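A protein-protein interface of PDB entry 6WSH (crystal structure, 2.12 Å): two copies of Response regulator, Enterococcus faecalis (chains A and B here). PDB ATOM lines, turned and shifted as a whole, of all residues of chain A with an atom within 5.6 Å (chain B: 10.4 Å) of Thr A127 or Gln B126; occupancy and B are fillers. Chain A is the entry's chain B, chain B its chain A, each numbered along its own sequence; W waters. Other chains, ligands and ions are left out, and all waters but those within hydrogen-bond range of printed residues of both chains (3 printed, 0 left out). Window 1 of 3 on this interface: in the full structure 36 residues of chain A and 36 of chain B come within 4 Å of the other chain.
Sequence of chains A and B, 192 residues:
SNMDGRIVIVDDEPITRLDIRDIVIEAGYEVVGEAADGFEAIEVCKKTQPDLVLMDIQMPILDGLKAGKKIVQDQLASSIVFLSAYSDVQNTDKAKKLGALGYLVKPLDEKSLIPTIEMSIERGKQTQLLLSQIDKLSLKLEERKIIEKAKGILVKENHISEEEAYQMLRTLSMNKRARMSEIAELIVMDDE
The side-chain amino group of Lys B96 is in salt-bridge range of the side-chain carboxylate of Glu A122, 3.7 Å away. The backbone carbonyl oxygen (O) of Lys B96 lies within hydrogen-bond range of the guanidinium group (NH1) of Arg A123, 2.9 Å away. The backbone carbonyl oxygen (O) of Ala B100 sits at hydrogen-bond distance from the guanidinium group (NH1) of Arg A123 (2.8 Å).
OE1 of Gln B126 sits at hydrogen-bond distance from NH2 of Arg B123 (2.8 Å). OE1 of Gln A126 sits at hydrogen-bond distance from NE of Arg A123 (2.8 Å). O of Arg A123 sits at hydrogen-bond distance from OG1 of Thr A127. The backbone carbonyl oxygen of Arg B123 sits at hydrogen-bond distance from the side-chain hydroxyl of Thr B127, at 2.8 Å.
Among the printed residues, pairs that only touch across the chains: Arg A123 with Gly B99, Gly A99 with Arg B123, Arg A123 with Leu B101, Leu A101 with Arg B123, Leu A130 with Ile B134, Leu A101 with Leu B101, Leu A131 with Leu B130, Leu A130 with Leu B131, Thr A127 with Gln B126 and Thr A127 with Leu B130.
Gly A99 touches just one residue of chain B: Arg B123 (3.3 Å). Printed residues of chain B within 4 Å of Leu A101: Leu B101 and Arg B123. Of the printed residues of chain B, Glu A122 touches Lys B96 (3.2 Å). Of the printed residues of chain B, Arg A123 touches Lys B96 (2.9 Å), Gly B99 (3.2 Å), Ala B100 (2.8 Å) and Leu B101 (3.4 Å). No residue of chain B comes within 4 Å of Gly A124. No residue of chain B comes within 4 Å of Gln A126. Of the printed residues of chain B, Thr A127 touches Gln B126 and Leu B130. Printed residues of chain B within 4 Å of Leu A131: Leu B130 (3.9 Å). Of the printed residues of chain A, Gly B99 touches Arg A123. Gln B126 touches just one residue of chain A: Thr A127 (3.96 Å). Printed residues of chain A within 4 Å of Ile B134: Leu A130 (3.5 Å). The nearest residue of chain A that does not touch Gln B126 is Gly A99 (5.1 Å). The nearest printed residue of chain A that does not touch Leu B131 is Gln A126 (5.4 Å).
Hydrophobic or aromatic side chains of chain B within 4 Å of the printed part of chain A: Leu B101, Leu B130, Leu B131 and Ile B134. Of the 13 printed residues of chain A, 7 touch a printed residue of chain B. Among the printed residues, 13 pairs touch across the chains. Among the printed residues, Asp or Glu carboxylates within 4 Å of a Lys or Arg side-chain nitrogen of the other chain: Glu A122 with Lys B96 (3.7 Å).
Leu B101 touches its own counterpart, Leu A101. Thr A127 touches Gln B126, but with the chains exchanged Gln A126 does not touch Thr B127 (4.2 Å). Thr A127 touches Leu B130, but with the chains exchanged Leu A130 does not touch Thr B127 (4.2 Å). Leu A130 touches Leu B131, and with the chains exchanged Leu A131 touches Leu B130. Of the 13 pairs that touch across the chains among the printed residues, 7 have their exchanged pair printed and touching as well.
Water W2 lies within hydrogen-bond range of the side-chain hydroxyl of Thr A127 (2.8 Å) and the side-chain hydroxyl of Thr B127 (2.8 Å). Water W1 bridges the backbone carbonyl oxygen of Leu B101 and the backbone carbonyl oxygen of Leu A101. Water W3 lies within hydrogen-bond range of the backbone carbonyl oxygen of Leu B101 and the backbone carbonyl oxygen of Leu A101.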
ATOM      1  N   GLY A  99      24.851 -13.464  24.694  1.00  0.00           N
ATOM      2  CA  GLY A  99      24.647 -12.102  24.222  1.00  0.00           C
ATOM      3  C   GLY A  99      24.561 -11.813  22.735  1.00  0.00           C
ATOM      4  O   GLY A  99      24.518 -10.650  22.318  1.00  0.00           O
ATOM      5  N   LEU A 101      23.358 -11.285  18.941  1.00  0.00           N
ATOM      6  CA  LEU A 101      22.324 -10.439  18.371  1.00  0.00           C
ATOM      7  C   LEU A 101      21.672 -11.080  17.146  1.00  0.00           C
ATOM      8  O   LEU A 101      20.618 -10.608  16.699  1.00  0.00           O
ATOM      9  CB  LEU A 101      22.942  -9.089  17.990  1.00  0.00           C
ATOM     10  CG  LEU A 101      22.920  -8.143  19.192  1.00  0.00           C
ATOM     11  CD1 LEU A 101      23.915  -6.993  19.123  1.00  0.00           C
ATOM     12  CD2 LEU A 101      21.510  -7.593  19.406  1.00  0.00           C
ATOM     13  N   GLU A 122      24.100  -1.995  14.681  1.00  0.00           N
ATOM     14  CA  GLU A 122      23.449  -0.864  15.337  1.00  0.00           C
ATOM     15  C   GLU A 122      23.030  -1.217  16.765  1.00  0.00           C
ATOM     16  O   GLU A 122      23.281  -0.447  17.704  1.00  0.00           O
ATOM     17  CB  GLU A 122      22.257  -0.420  14.515  1.00  0.00           C
ATOM     18  CG  GLU A 122      21.644   0.923  14.841  1.00  0.00           C
ATOM     19  CD  GLU A 122      22.484   2.102  14.440  1.00  0.00           C
ATOM     20  OE1 GLU A 122      22.682   2.994  15.302  1.00  0.00           O
ATOM     21  OE2 GLU A 122      23.060   2.041  13.341  1.00  0.00           O
ATOM     22  N   ARG A 123      22.388  -2.375  16.951  1.00  0.00           N
ATOM     23  CA  ARG A 123      21.947  -2.779  18.281  1.00  0.00           C
ATOM     24  C   ARG A 123      23.120  -2.986  19.242  1.00  0.00           C
ATOM     25  O   ARG A 123      23.037  -2.614  20.422  1.00  0.00           O
ATOM     26  CB  ARG A 123      21.109  -4.061  18.167  1.00  0.00           C
ATOM     27  CG  ARG A 123      19.795  -3.888  17.374  1.00  0.00           C
ATOM     28  CD  ARG A 123      18.648  -3.290  18.216  1.00  0.00           C
ATOM     29  NE  ARG A 123      18.833  -1.856  18.409  1.00  0.00           N
ATOM     30  CZ  ARG A 123      18.709  -0.945  17.452  1.00  0.00           C
ATOM     31  NH1 ARG A 123      18.322  -1.304  16.235  1.00  0.00           N
ATOM     32  NH2 ARG A 123      18.937   0.334  17.726  1.00  0.00           N
ATOM     33  N   GLY A 124      24.218  -3.579  18.770  1.00  0.00           N
ATOM     34  CA  GLY A 124      25.379  -3.740  19.626  1.00  0.00           C
ATOM     35  C   GLY A 124      25.945  -2.426  20.122  1.00  0.00           C
ATOM     36  O   GLY A 124      26.275  -2.281  21.310  1.00  0.00           O
ATOM     37  N   LYS A 125      26.085  -1.453  19.221  1.00  0.00           N
ATOM     38  CA  LYS A 125      26.609  -0.165  19.671  1.00  0.00           C
ATOM     39  C   LYS A 125      25.617   0.566  20.586  1.00  0.00           C
ATOM     40  O   LYS A 125      26.027   1.228  21.558  1.00  0.00           O
ATOM     41  CB  LYS A 125      27.036   0.671  18.461  1.00  0.00           C
ATOM     42  CG  LYS A 125      28.194  -0.023  17.697  1.00  0.00           C
ATOM     43  CD  LYS A 125      28.883   0.815  16.611  1.00  0.00           C
ATOM     44  CE  LYS A 125      30.228   1.365  17.096  1.00  0.00           C
ATOM     45  NZ  LYS A 125      31.325   0.348  17.204  1.00  0.00           N
ATOM     46  N   GLN A 126      24.311   0.430  20.326  1.00  0.00           N
ATOM     47  CA  GLN A 126      23.337   0.942  21.291  1.00  0.00           C
ATOM     48  C   GLN A 126      23.535   0.318  22.673  1.00  0.00           C
ATOM     49  O   GLN A 126      23.521   1.021  23.703  1.00  0.00           O
ATOM     50  CB  GLN A 126      21.914   0.698  20.792  1.00  0.00           C
ATOM     51  CG  GLN A 126      20.812   1.254  21.715  1.00  0.00           C
ATOM     52  CD  GLN A 126      19.443   0.593  21.504  1.00  0.00           C
ATOM     53  OE1 GLN A 126      19.273  -0.270  20.643  1.00  0.00           O
ATOM     54  NE2 GLN A 126      18.452   0.986  22.292  1.00  0.00           N
ATOM     55  N   THR A 127      23.715  -1.001  22.714  1.00  0.00           N
ATOM     56  CA  THR A 127      23.866  -1.677  23.992  1.00  0.00           C
ATOM     57  C   THR A 127      25.125  -1.222  24.722  1.00  0.00           C
ATOM     58  O   THR A 127      25.120  -1.049  25.951  1.00  0.00           O
ATOM     59  CB  THR A 127      23.895  -3.184  23.774  1.00  0.00           C
ATOM     60  OG1 THR A 127      22.700  -3.576  23.069  1.00  0.00           O
ATOM     61  CG2 THR A 127      23.977  -3.897  25.113  1.00  0.00           C
ATOM     62  N   GLN A 128      26.225  -1.068  23.989  1.00  0.00           N
ATOM     63  CA  GLN A 128      27.443  -0.564  24.607  1.00  0.00           C
ATOM     64  C   GLN A 128      27.220   0.813  25.214  1.00  0.00           C
ATOM     65  O   GLN A 128      27.645   1.079  26.352  1.00  0.00           O
ATOM     66  CB  GLN A 128      28.559  -0.526  23.570  1.00  0.00           C
ATOM     67  CG  GLN A 128      29.031  -1.915  23.096  1.00  0.00           C
ATOM     68  CD  GLN A 128      30.267  -1.879  22.222  1.00  0.00           C
ATOM     69  OE1 GLN A 128      30.395  -1.039  21.329  1.00  0.00           O
ATOM     70  NE2 GLN A 128      31.195  -2.803  22.466  1.00  0.00           N
ATOM     71  N   LEU A 129      26.524   1.695  24.493  1.00  0.00           N
ATOM     72  CA  LEU A 129      26.218   3.004  25.064  1.00  0.00           C
ATOM     73  C   LEU A 129      25.410   2.879  26.358  1.00  0.00           C
ATOM     74  O   LEU A 129      25.689   3.573  27.352  1.00  0.00           O
ATOM     75  CB  LEU A 129      25.492   3.865  24.028  1.00  0.00           C
ATOM     76  CG  LEU A 129      25.020   5.260  24.410  1.00  0.00           C
ATOM     77  CD1 LEU A 129      25.043   6.171  23.187  1.00  0.00           C
ATOM     78  CD2 LEU A 129      23.630   5.194  24.992  1.00  0.00           C
ATOM     79  N   LEU A 130      24.365   2.046  26.346  1.00  0.00           N
ATOM     80  CA  LEU A 130      23.547   1.922  27.552  1.00  0.00           C
ATOM     81  C   LEU A 130      24.346   1.390  28.747  1.00  0.00           C
ATOM     82  O   LEU A 130      24.156   1.845  29.893  1.00  0.00           O
ATOM     83  CB  LEU A 130      22.348   1.023  27.275  1.00  0.00           C
ATOM     84  CG  LEU A 130      21.329   1.525  26.250  1.00  0.00           C
ATOM     85  CD1 LEU A 130      20.199   0.517  26.031  1.00  0.00           C
ATOM     86  CD2 LEU A 130      20.756   2.873  26.676  1.00  0.00           C
ATOM     87  N   LEU A 131      25.233   0.414  28.506  1.00  0.00           N
ATOM     88  CA  LEU A 131      26.060  -0.094  29.601  1.00  0.00           C
ATOM     89  C   LEU A 131      27.027   0.967  30.123  1.00  0.00           C
ATOM     90  O   LEU A 131      27.270   1.047  31.342  1.00  0.00           O
ATOM     91  CB  LEU A 131      26.826  -1.327  29.131  1.00  0.00           C
ATOM     92  CG  LEU A 131      25.967  -2.567  28.862  1.00  0.00           C
ATOM     93  CD1 LEU A 131      26.762  -3.688  28.216  1.00  0.00           C
ATOM     94  CD2 LEU A 131      25.321  -3.067  30.154  1.00  0.00           C
ATOM     95  N   SER A 132      27.525   1.830  29.238  1.00  0.00           N
ATOM     96  CA  SER A 132      28.364   2.924  29.705  1.00  0.00           C
ATOM     97  C   SER A 132      27.574   3.916  30.554  1.00  0.00           C
ATOM     98  O   SER A 132      28.066   4.387  31.600  1.00  0.00           O
ATOM     99  CB  SER A 132      29.006   3.616  28.515  1.00  0.00           C
ATOM    100  OG  SER A 132      29.788   4.733  28.896  1.00  0.00           O
ATOM    101  N   ASP B  51       6.013  -9.986  23.429  1.00  0.00           N
ATOM    102  CA  ASP B  51       7.475 -10.038  23.489  1.00  0.00           C
ATOM    103  C   ASP B  51       8.136  -9.711  22.146  1.00  0.00           C
ATOM    104  O   ASP B  51       9.231  -9.129  22.114  1.00  0.00           O
ATOM    105  CB  ASP B  51       7.934 -11.427  23.947  1.00  0.00           C
ATOM    106  CG  ASP B  51       7.250 -11.895  25.207  1.00  0.00           C
ATOM    107  OD1 ASP B  51       6.739 -13.044  25.186  1.00  0.00           O
ATOM    108  OD2 ASP B  51       7.141 -11.118  26.155  1.00  0.00           O
ATOM    109  N   GLN B  75       6.981   1.892  23.736  1.00  0.00           N
ATOM    110  CA  GLN B  75       7.272   0.568  24.312  1.00  0.00           C
ATOM    111  C   GLN B  75       6.092  -0.402  24.290  1.00  0.00           C
ATOM    112  O   GLN B  75       5.762  -1.044  25.295  1.00  0.00           O
ATOM    113  CB  GLN B  75       7.858   0.693  25.731  1.00  0.00           C
ATOM    114  CG  GLN B  75       9.235   1.372  25.753  1.00  0.00           C
ATOM    115  CD  GLN B  75       9.927   1.407  27.130  1.00  0.00           C
ATOM    116  OE1 GLN B  75      10.037   0.392  27.827  1.00  0.00           O
ATOM    117  NE2 GLN B  75      10.470   2.560  27.499  1.00  0.00           N
ATOM    118  N   ALA B  77       5.965  -3.099  22.398  1.00  0.00           N
ATOM    119  CA  ALA B  77       6.454  -4.469  22.276  1.00  0.00           C
ATOM    120  C   ALA B  77       7.899  -4.489  22.756  1.00  0.00           C
ATOM    121  O   ALA B  77       8.587  -3.462  22.740  1.00  0.00           O
ATOM    122  CB  ALA B  77       6.370  -5.010  20.840  1.00  0.00           C
ATOM    123  N   SER B  78       8.348  -5.656  23.219  1.00  0.00           N
ATOM    124  CA  SER B  78       9.739  -5.757  23.648  1.00  0.00           C
ATOM    125  C   SER B  78      10.737  -5.857  22.488  1.00  0.00           C
ATOM    126  O   SER B  78      11.901  -5.471  22.659  1.00  0.00           O
ATOM    127  CB  SER B  78       9.902  -6.952  24.598  1.00  0.00           C
ATOM    128  OG  SER B  78       9.084  -6.840  25.757  1.00  0.00           O
ATOM    129  N   SER B  79      10.343  -6.390  21.328  1.00  0.00           N
ATOM    130  CA  SER B  79      11.261  -6.446  20.193  1.00  0.00           C
ATOM    131  C   SER B  79      10.491  -6.393  18.883  1.00  0.00           C
ATOM    132  O   SER B  79       9.316  -6.769  18.830  1.00  0.00           O
ATOM    133  CB  SER B  79      12.130  -7.704  20.252  1.00  0.00           C
ATOM    134  OG  SER B  79      11.339  -8.864  20.065  1.00  0.00           O
ATOM    135  N   LYS B  96      17.058  -0.114  11.319  1.00  0.00           N
ATOM    136  CA  LYS B  96      18.038  -0.144  12.393  1.00  0.00           C
ATOM    137  C   LYS B  96      17.930   1.090  13.277  1.00  0.00           C
ATOM    138  O   LYS B  96      18.011   0.974  14.513  1.00  0.00           O
ATOM    139  CB  LYS B  96      19.438  -0.323  11.806  1.00  0.00           C
ATOM    140  CG  LYS B  96      20.096   0.917  11.239  1.00  0.00           C
ATOM    141  CD  LYS B  96      21.422   0.522  10.588  1.00  0.00           C
ATOM    142  CE  LYS B  96      22.279   1.733  10.268  1.00  0.00           C
ATOM    143  NZ  LYS B  96      23.637   1.400   9.767  1.00  0.00           N
ATOM    144  N   GLY B  99      15.090   0.993  15.741  1.00  0.00           N
ATOM    145  CA  GLY B  99      15.464   0.113  16.834  1.00  0.00           C
ATOM    146  C   GLY B  99      15.138  -1.362  16.731  1.00  0.00           C
ATOM    147  O   GLY B  99      15.055  -2.058  17.747  1.00  0.00           O
ATOM    148  N   ALA B 100      14.956  -1.839  15.508  1.00  0.00           N
ATOM    149  CA  ALA B 100      14.710  -3.250  15.264  1.00  0.00           C
ATOM    150  C   ALA B 100      15.905  -4.112  15.656  1.00  0.00           C
ATOM    151  O   ALA B 100      17.067  -3.710  15.552  1.00  0.00           O
ATOM    152  CB  ALA B 100      14.391  -3.472  13.789  1.00  0.00           C
ATOM    153  N   LEU B 101      15.582  -5.327  16.099  1.00  0.00           N
ATOM    154  CA  LEU B 101      16.545  -6.337  16.501  1.00  0.00           C
ATOM    155  C   LEU B 101      16.810  -7.372  15.406  1.00  0.00           C
ATOM    156  O   LEU B 101      17.806  -8.104  15.494  1.00  0.00           O
ATOM    157  CB  LEU B 101      16.040  -7.047  17.763  1.00  0.00           C
ATOM    158  CG  LEU B 101      16.466  -6.300  19.029  1.00  0.00           C
ATOM    159  CD1 LEU B 101      15.715  -6.700  20.294  1.00  0.00           C
ATOM    160  CD2 LEU B 101      17.966  -6.430  19.260  1.00  0.00           C
ATOM    161  N   GLU B 118      14.231 -16.324  18.887  1.00  0.00           N
ATOM    162  CA  GLU B 118      14.809 -16.511  20.215  1.00  0.00           C
ATOM    163  C   GLU B 118      15.809 -15.411  20.572  1.00  0.00           C
ATOM    164  O   GLU B 118      15.727 -14.785  21.652  1.00  0.00           O
ATOM    165  CB  GLU B 118      15.477 -17.876  20.293  1.00  0.00           C
ATOM    166  CG  GLU B 118      14.523 -19.057  20.401  1.00  0.00           C
ATOM    167  CD  GLU B 118      13.759 -19.047  21.692  1.00  0.00           C
ATOM    168  OE1 GLU B 118      14.418 -19.213  22.742  1.00  0.00           O
ATOM    169  OE2 GLU B 118      12.531 -18.847  21.659  1.00  0.00           O
ATOM    170  N   MET B 119      16.732 -15.122  19.655  1.00  0.00           N
ATOM    171  CA  MET B 119      17.669 -14.035  19.901  1.00  0.00           C
ATOM    172  C   MET B 119      16.962 -12.705  20.152  1.00  0.00           C
ATOM    173  O   MET B 119      17.320 -11.970  21.088  1.00  0.00           O
ATOM    174  CB  MET B 119      18.609 -13.895  18.711  1.00  0.00           C
ATOM    175  CG  MET B 119      19.371 -15.139  18.269  1.00  0.00           C
ATOM    176  SD  MET B 119      20.226 -16.093  19.550  1.00  0.00           S
ATOM    177  CE  MET B 119      21.414 -14.877  20.120  1.00  0.00           C
ATOM    178  N   SER B 120      16.015 -12.341  19.282  1.00  0.00           N
ATOM    179  CA  SER B 120      15.395 -11.030  19.388  1.00  0.00           C
ATOM    180  C   SER B 120      14.585 -10.866  20.673  1.00  0.00           C
ATOM    181  O   SER B 120      14.619  -9.794  21.301  1.00  0.00           O
ATOM    182  CB  SER B 120      14.508 -10.795  18.167  1.00  0.00           C
ATOM    183  OG  SER B 120      15.242 -10.901  16.952  1.00  0.00           O
ATOM    184  N   ILE B 121      13.875 -11.907  21.101  1.00  0.00           N
ATOM    185  CA  ILE B 121      13.152 -11.799  22.366  1.00  0.00           C
ATOM    186  C   ILE B 121      14.131 -11.616  23.523  1.00  0.00           C
ATOM    187  O   ILE B 121      13.927 -10.757  24.405  1.00  0.00           O
ATOM    188  CB  ILE B 121      12.241 -13.028  22.552  1.00  0.00           C
ATOM    189  CG1 ILE B 121      11.082 -12.944  21.551  1.00  0.00           C
ATOM    190  CG2 ILE B 121      11.714 -13.095  23.970  1.00  0.00           C
ATOM    191  CD1 ILE B 121      10.193 -14.172  21.509  1.00  0.00           C
ATOM    192  N   GLU B 122      15.216 -12.400  23.537  1.00  0.00           N
ATOM    193  CA  GLU B 122      16.163 -12.277  24.639  1.00  0.00           C
ATOM    194  C   GLU B 122      16.787 -10.880  24.679  1.00  0.00           C
ATOM    195  O   GLU B 122      16.879 -10.245  25.748  1.00  0.00           O
ATOM    196  CB  GLU B 122      17.252 -13.336  24.496  1.00  0.00           C
ATOM    197  CG  GLU B 122      18.304 -13.385  25.603  1.00  0.00           C
ATOM    198  CD  GLU B 122      17.790 -13.927  26.910  1.00  0.00           C
ATOM    199  OE1 GLU B 122      16.784 -14.660  26.890  1.00  0.00           O
ATOM    200  OE2 GLU B 122      18.420 -13.635  27.948  1.00  0.00           O
ATOM    201  N   ARG B 123      17.244 -10.394  23.516  1.00  0.00           N
ATOM    202  CA  ARG B 123      17.862  -9.071  23.439  1.00  0.00           C
ATOM    203  C   ARG B 123      16.875  -7.957  23.802  1.00  0.00           C
ATOM    204  O   ARG B 123      17.258  -6.980  24.464  1.00  0.00           O
ATOM    205  CB  ARG B 123      18.443  -8.866  22.034  1.00  0.00           C
ATOM    206  CG  ARG B 123      19.647  -9.768  21.660  1.00  0.00           C
ATOM    207  CD  ARG B 123      20.992  -9.343  22.283  1.00  0.00           C
ATOM    208  NE  ARG B 123      21.099  -9.729  23.675  1.00  0.00           N
ATOM    209  CZ  ARG B 123      21.209 -10.971  24.105  1.00  0.00           C
ATOM    210  NH1 ARG B 123      21.350 -11.970  23.249  1.00  0.00           N
ATOM    211  NH2 ARG B 123      21.261 -11.207  25.402  1.00  0.00           N
ATOM    212  N   GLY B 124      15.605  -8.085  23.398  1.00  0.00           N
ATOM    213  CA  GLY B 124      14.631  -7.069  23.753  1.00  0.00           C
ATOM    214  C   GLY B 124      14.375  -6.977  25.247  1.00  0.00           C
ATOM    215  O   GLY B 124      14.318  -5.876  25.825  1.00  0.00           O
ATOM    216  N   LYS B 125      14.210  -8.133  25.893  1.00  0.00           N
ATOM    217  CA  LYS B 125      14.026  -8.128  27.339  1.00  0.00           C
ATOM    218  C   LYS B 125      15.258  -7.579  28.065  1.00  0.00           C
ATOM    219  O   LYS B 125      15.138  -6.761  29.000  1.00  0.00           O
ATOM    220  CB  LYS B 125      13.701  -9.548  27.783  1.00  0.00           C
ATOM    221  CG  LYS B 125      12.322 -10.088  27.327  1.00  0.00           C
ATOM    222  CD  LYS B 125      11.127  -9.439  28.011  1.00  0.00           C
ATOM    223  CE  LYS B 125      11.192  -9.618  29.537  1.00  0.00           C
ATOM    224  NZ  LYS B 125       9.893  -9.330  30.222  1.00  0.00           N
ATOM    225  N   GLN B 126      16.456  -7.986  27.630  1.00  0.00           N
ATOM    226  CA  GLN B 126      17.675  -7.384  28.175  1.00  0.00           C
ATOM    227  C   GLN B 126      17.680  -5.859  28.042  1.00  0.00           C
ATOM    228  O   GLN B 126      17.977  -5.134  29.012  1.00  0.00           O
ATOM    229  CB  GLN B 126      18.884  -8.007  27.485  1.00  0.00           C
ATOM    230  CG  GLN B 126      20.224  -7.344  27.783  1.00  0.00           C
ATOM    231  CD  GLN B 126      21.406  -7.935  26.998  1.00  0.00           C
ATOM    232  OE1 GLN B 126      21.757  -9.105  27.152  1.00  0.00           O
ATOM    233  NE2 GLN B 126      21.971  -7.167  26.083  1.00  0.00           N
ATOM    234  N   THR B 127      17.395  -5.355  26.841  1.00  0.00           N
ATOM    235  CA  THR B 127      17.444  -3.924  26.624  1.00  0.00           C
ATOM    236  C   THR B 127      16.434  -3.182  27.495  1.00  0.00           C
ATOM    237  O   THR B 127      16.724  -2.078  27.995  1.00  0.00           O
ATOM    238  CB  THR B 127      17.168  -3.635  25.141  1.00  0.00           C
ATOM    239  OG1 THR B 127      18.166  -4.305  24.351  1.00  0.00           O
ATOM    240  CG2 THR B 127      17.207  -2.147  24.873  1.00  0.00           C
ATOM    241  N   GLN B 128      15.218  -3.737  27.636  1.00  0.00           N
ATOM    242  CA  GLN B 128      14.270  -3.131  28.556  1.00  0.00           C
ATOM    243  C   GLN B 128      14.801  -3.082  29.981  1.00  0.00           C
ATOM    244  O   GLN B 128      14.599  -2.084  30.690  1.00  0.00           O
ATOM    245  CB  GLN B 128      12.957  -3.920  28.545  1.00  0.00           C
ATOM    246  CG  GLN B 128      12.075  -3.665  27.322  1.00  0.00           C
ATOM    247  CD  GLN B 128      10.771  -4.465  27.354  1.00  0.00           C
ATOM    248  OE1 GLN B 128       9.835  -4.182  26.617  1.00  0.00           O
ATOM    249  NE2 GLN B 128      10.623  -5.320  28.355  1.00  0.00           N
ATOM    250  N   LEU B 129      15.494  -4.132  30.425  1.00  0.00           N
ATOM    251  CA  LEU B 129      16.130  -4.058  31.747  1.00  0.00           C
ATOM    252  C   LEU B 129      17.161  -2.929  31.841  1.00  0.00           C
ATOM    253  O   LEU B 129      17.242  -2.215  32.854  1.00  0.00           O
ATOM    254  CB  LEU B 129      16.778  -5.393  32.102  1.00  0.00           C
ATOM    255  CG  LEU B 129      15.857  -6.601  32.255  1.00  0.00           C
ATOM    256  CD1 LEU B 129      16.648  -7.883  32.532  1.00  0.00           C
ATOM    257  CD2 LEU B 129      14.837  -6.334  33.356  1.00  0.00           C
ATOM    258  N   LEU B 130      18.015  -2.800  30.830  1.00  0.00           N
ATOM    259  CA  LEU B 130      19.003  -1.721  30.859  1.00  0.00           C
ATOM    260  C   LEU B 130      18.347  -0.341  30.943  1.00  0.00           C
ATOM    261  O   LEU B 130      18.765   0.528  31.733  1.00  0.00           O
ATOM    262  CB  LEU B 130      19.900  -1.809  29.629  1.00  0.00           C
ATOM    263  CG  LEU B 130      20.692  -3.096  29.393  1.00  0.00           C
ATOM    264  CD1 LEU B 130      21.611  -2.962  28.182  1.00  0.00           C
ATOM    265  CD2 LEU B 130      21.493  -3.462  30.631  1.00  0.00           C
ATOM    266  N   LEU B 131      17.359  -0.102  30.083  1.00  0.00           N
ATOM    267  CA  LEU B 131      16.635   1.164  30.103  1.00  0.00           C
ATOM    268  C   LEU B 131      15.950   1.432  31.444  1.00  0.00           C
ATOM    269  O   LEU B 131      15.977   2.568  31.955  1.00  0.00           O
ATOM    270  CB  LEU B 131      15.606   1.139  28.977  1.00  0.00           C
ATOM    271  CG  LEU B 131      16.170   1.147  27.555  1.00  0.00           C
ATOM    272  CD1 LEU B 131      15.099   0.977  26.487  1.00  0.00           C
ATOM    273  CD2 LEU B 131      16.943   2.434  27.302  1.00  0.00           C
ATOM    274  N   SER B 132      15.373   0.396  32.053  1.00  0.00           N
ATOM    275  CA  SER B 132      14.813   0.548  33.391  1.00  0.00           C
ATOM    276  C   SER B 132      15.869   0.919  34.425  1.00  0.00           C
ATOM    277  O   SER B 132      15.633   1.788  35.285  1.00  0.00           O
ATOM    278  CB  SER B 132      14.114  -0.752  33.781  1.00  0.00           C
ATOM    279  OG  SER B 132      13.499  -0.679  35.048  1.00  0.00           O
ATOM    280  N   GLN B 133      17.025   0.251  34.390  1.00  0.00           N
ATOM    281  CA  GLN B 133      18.086   0.613  35.324  1.00  0.00           C
ATOM    282  C   GLN B 133      18.526   2.064  35.140  1.00  0.00           C
ATOM    283  O   GLN B 133      18.757   2.789  36.124  1.00  0.00           O
ATOM    284  CB  GLN B 133      19.280  -0.328  35.170  1.00  0.00           C
ATOM    285  CG  GLN B 133      19.028  -1.763  35.642  1.00  0.00           C
ATOM    286  CD  GLN B 133      20.172  -2.732  35.291  1.00  0.00           C
ATOM    287  OE1 GLN B 133      21.331  -2.338  35.145  1.00  0.00           O
ATOM    288  NE2 GLN B 133      19.859  -4.012  35.165  1.00  0.00           N
ATOM    289  N   ILE B 134      18.694   2.493  33.887  1.00  0.00           N
ATOM    290  CA  ILE B 134      19.084   3.878  33.631  1.00  0.00           C
ATOM    291  C   ILE B 134      18.059   4.856  34.205  1.00  0.00           C
ATOM    292  O   ILE B 134      18.425   5.863  34.830  1.00  0.00           O
ATOM    293  CB  ILE B 134      19.288   4.091  32.121  1.00  0.00           C
ATOM    294  CG1 ILE B 134      20.512   3.314  31.634  1.00  0.00           C
ATOM    295  CG2 ILE B 134      19.429   5.570  31.817  1.00  0.00           C
ATOM    296  CD1 ILE B 134      20.541   3.113  30.126  1.00  0.00           C
HETATM  297  O   HOH W   1      20.193  -8.674  14.206  1.00  0.00           O
HETATM  298  O   HOH W   2      20.471  -2.748  24.479  1.00  0.00           O
HETATM  299  O   HOH W   3      18.696 -10.888  13.866  1.00  0.00           O
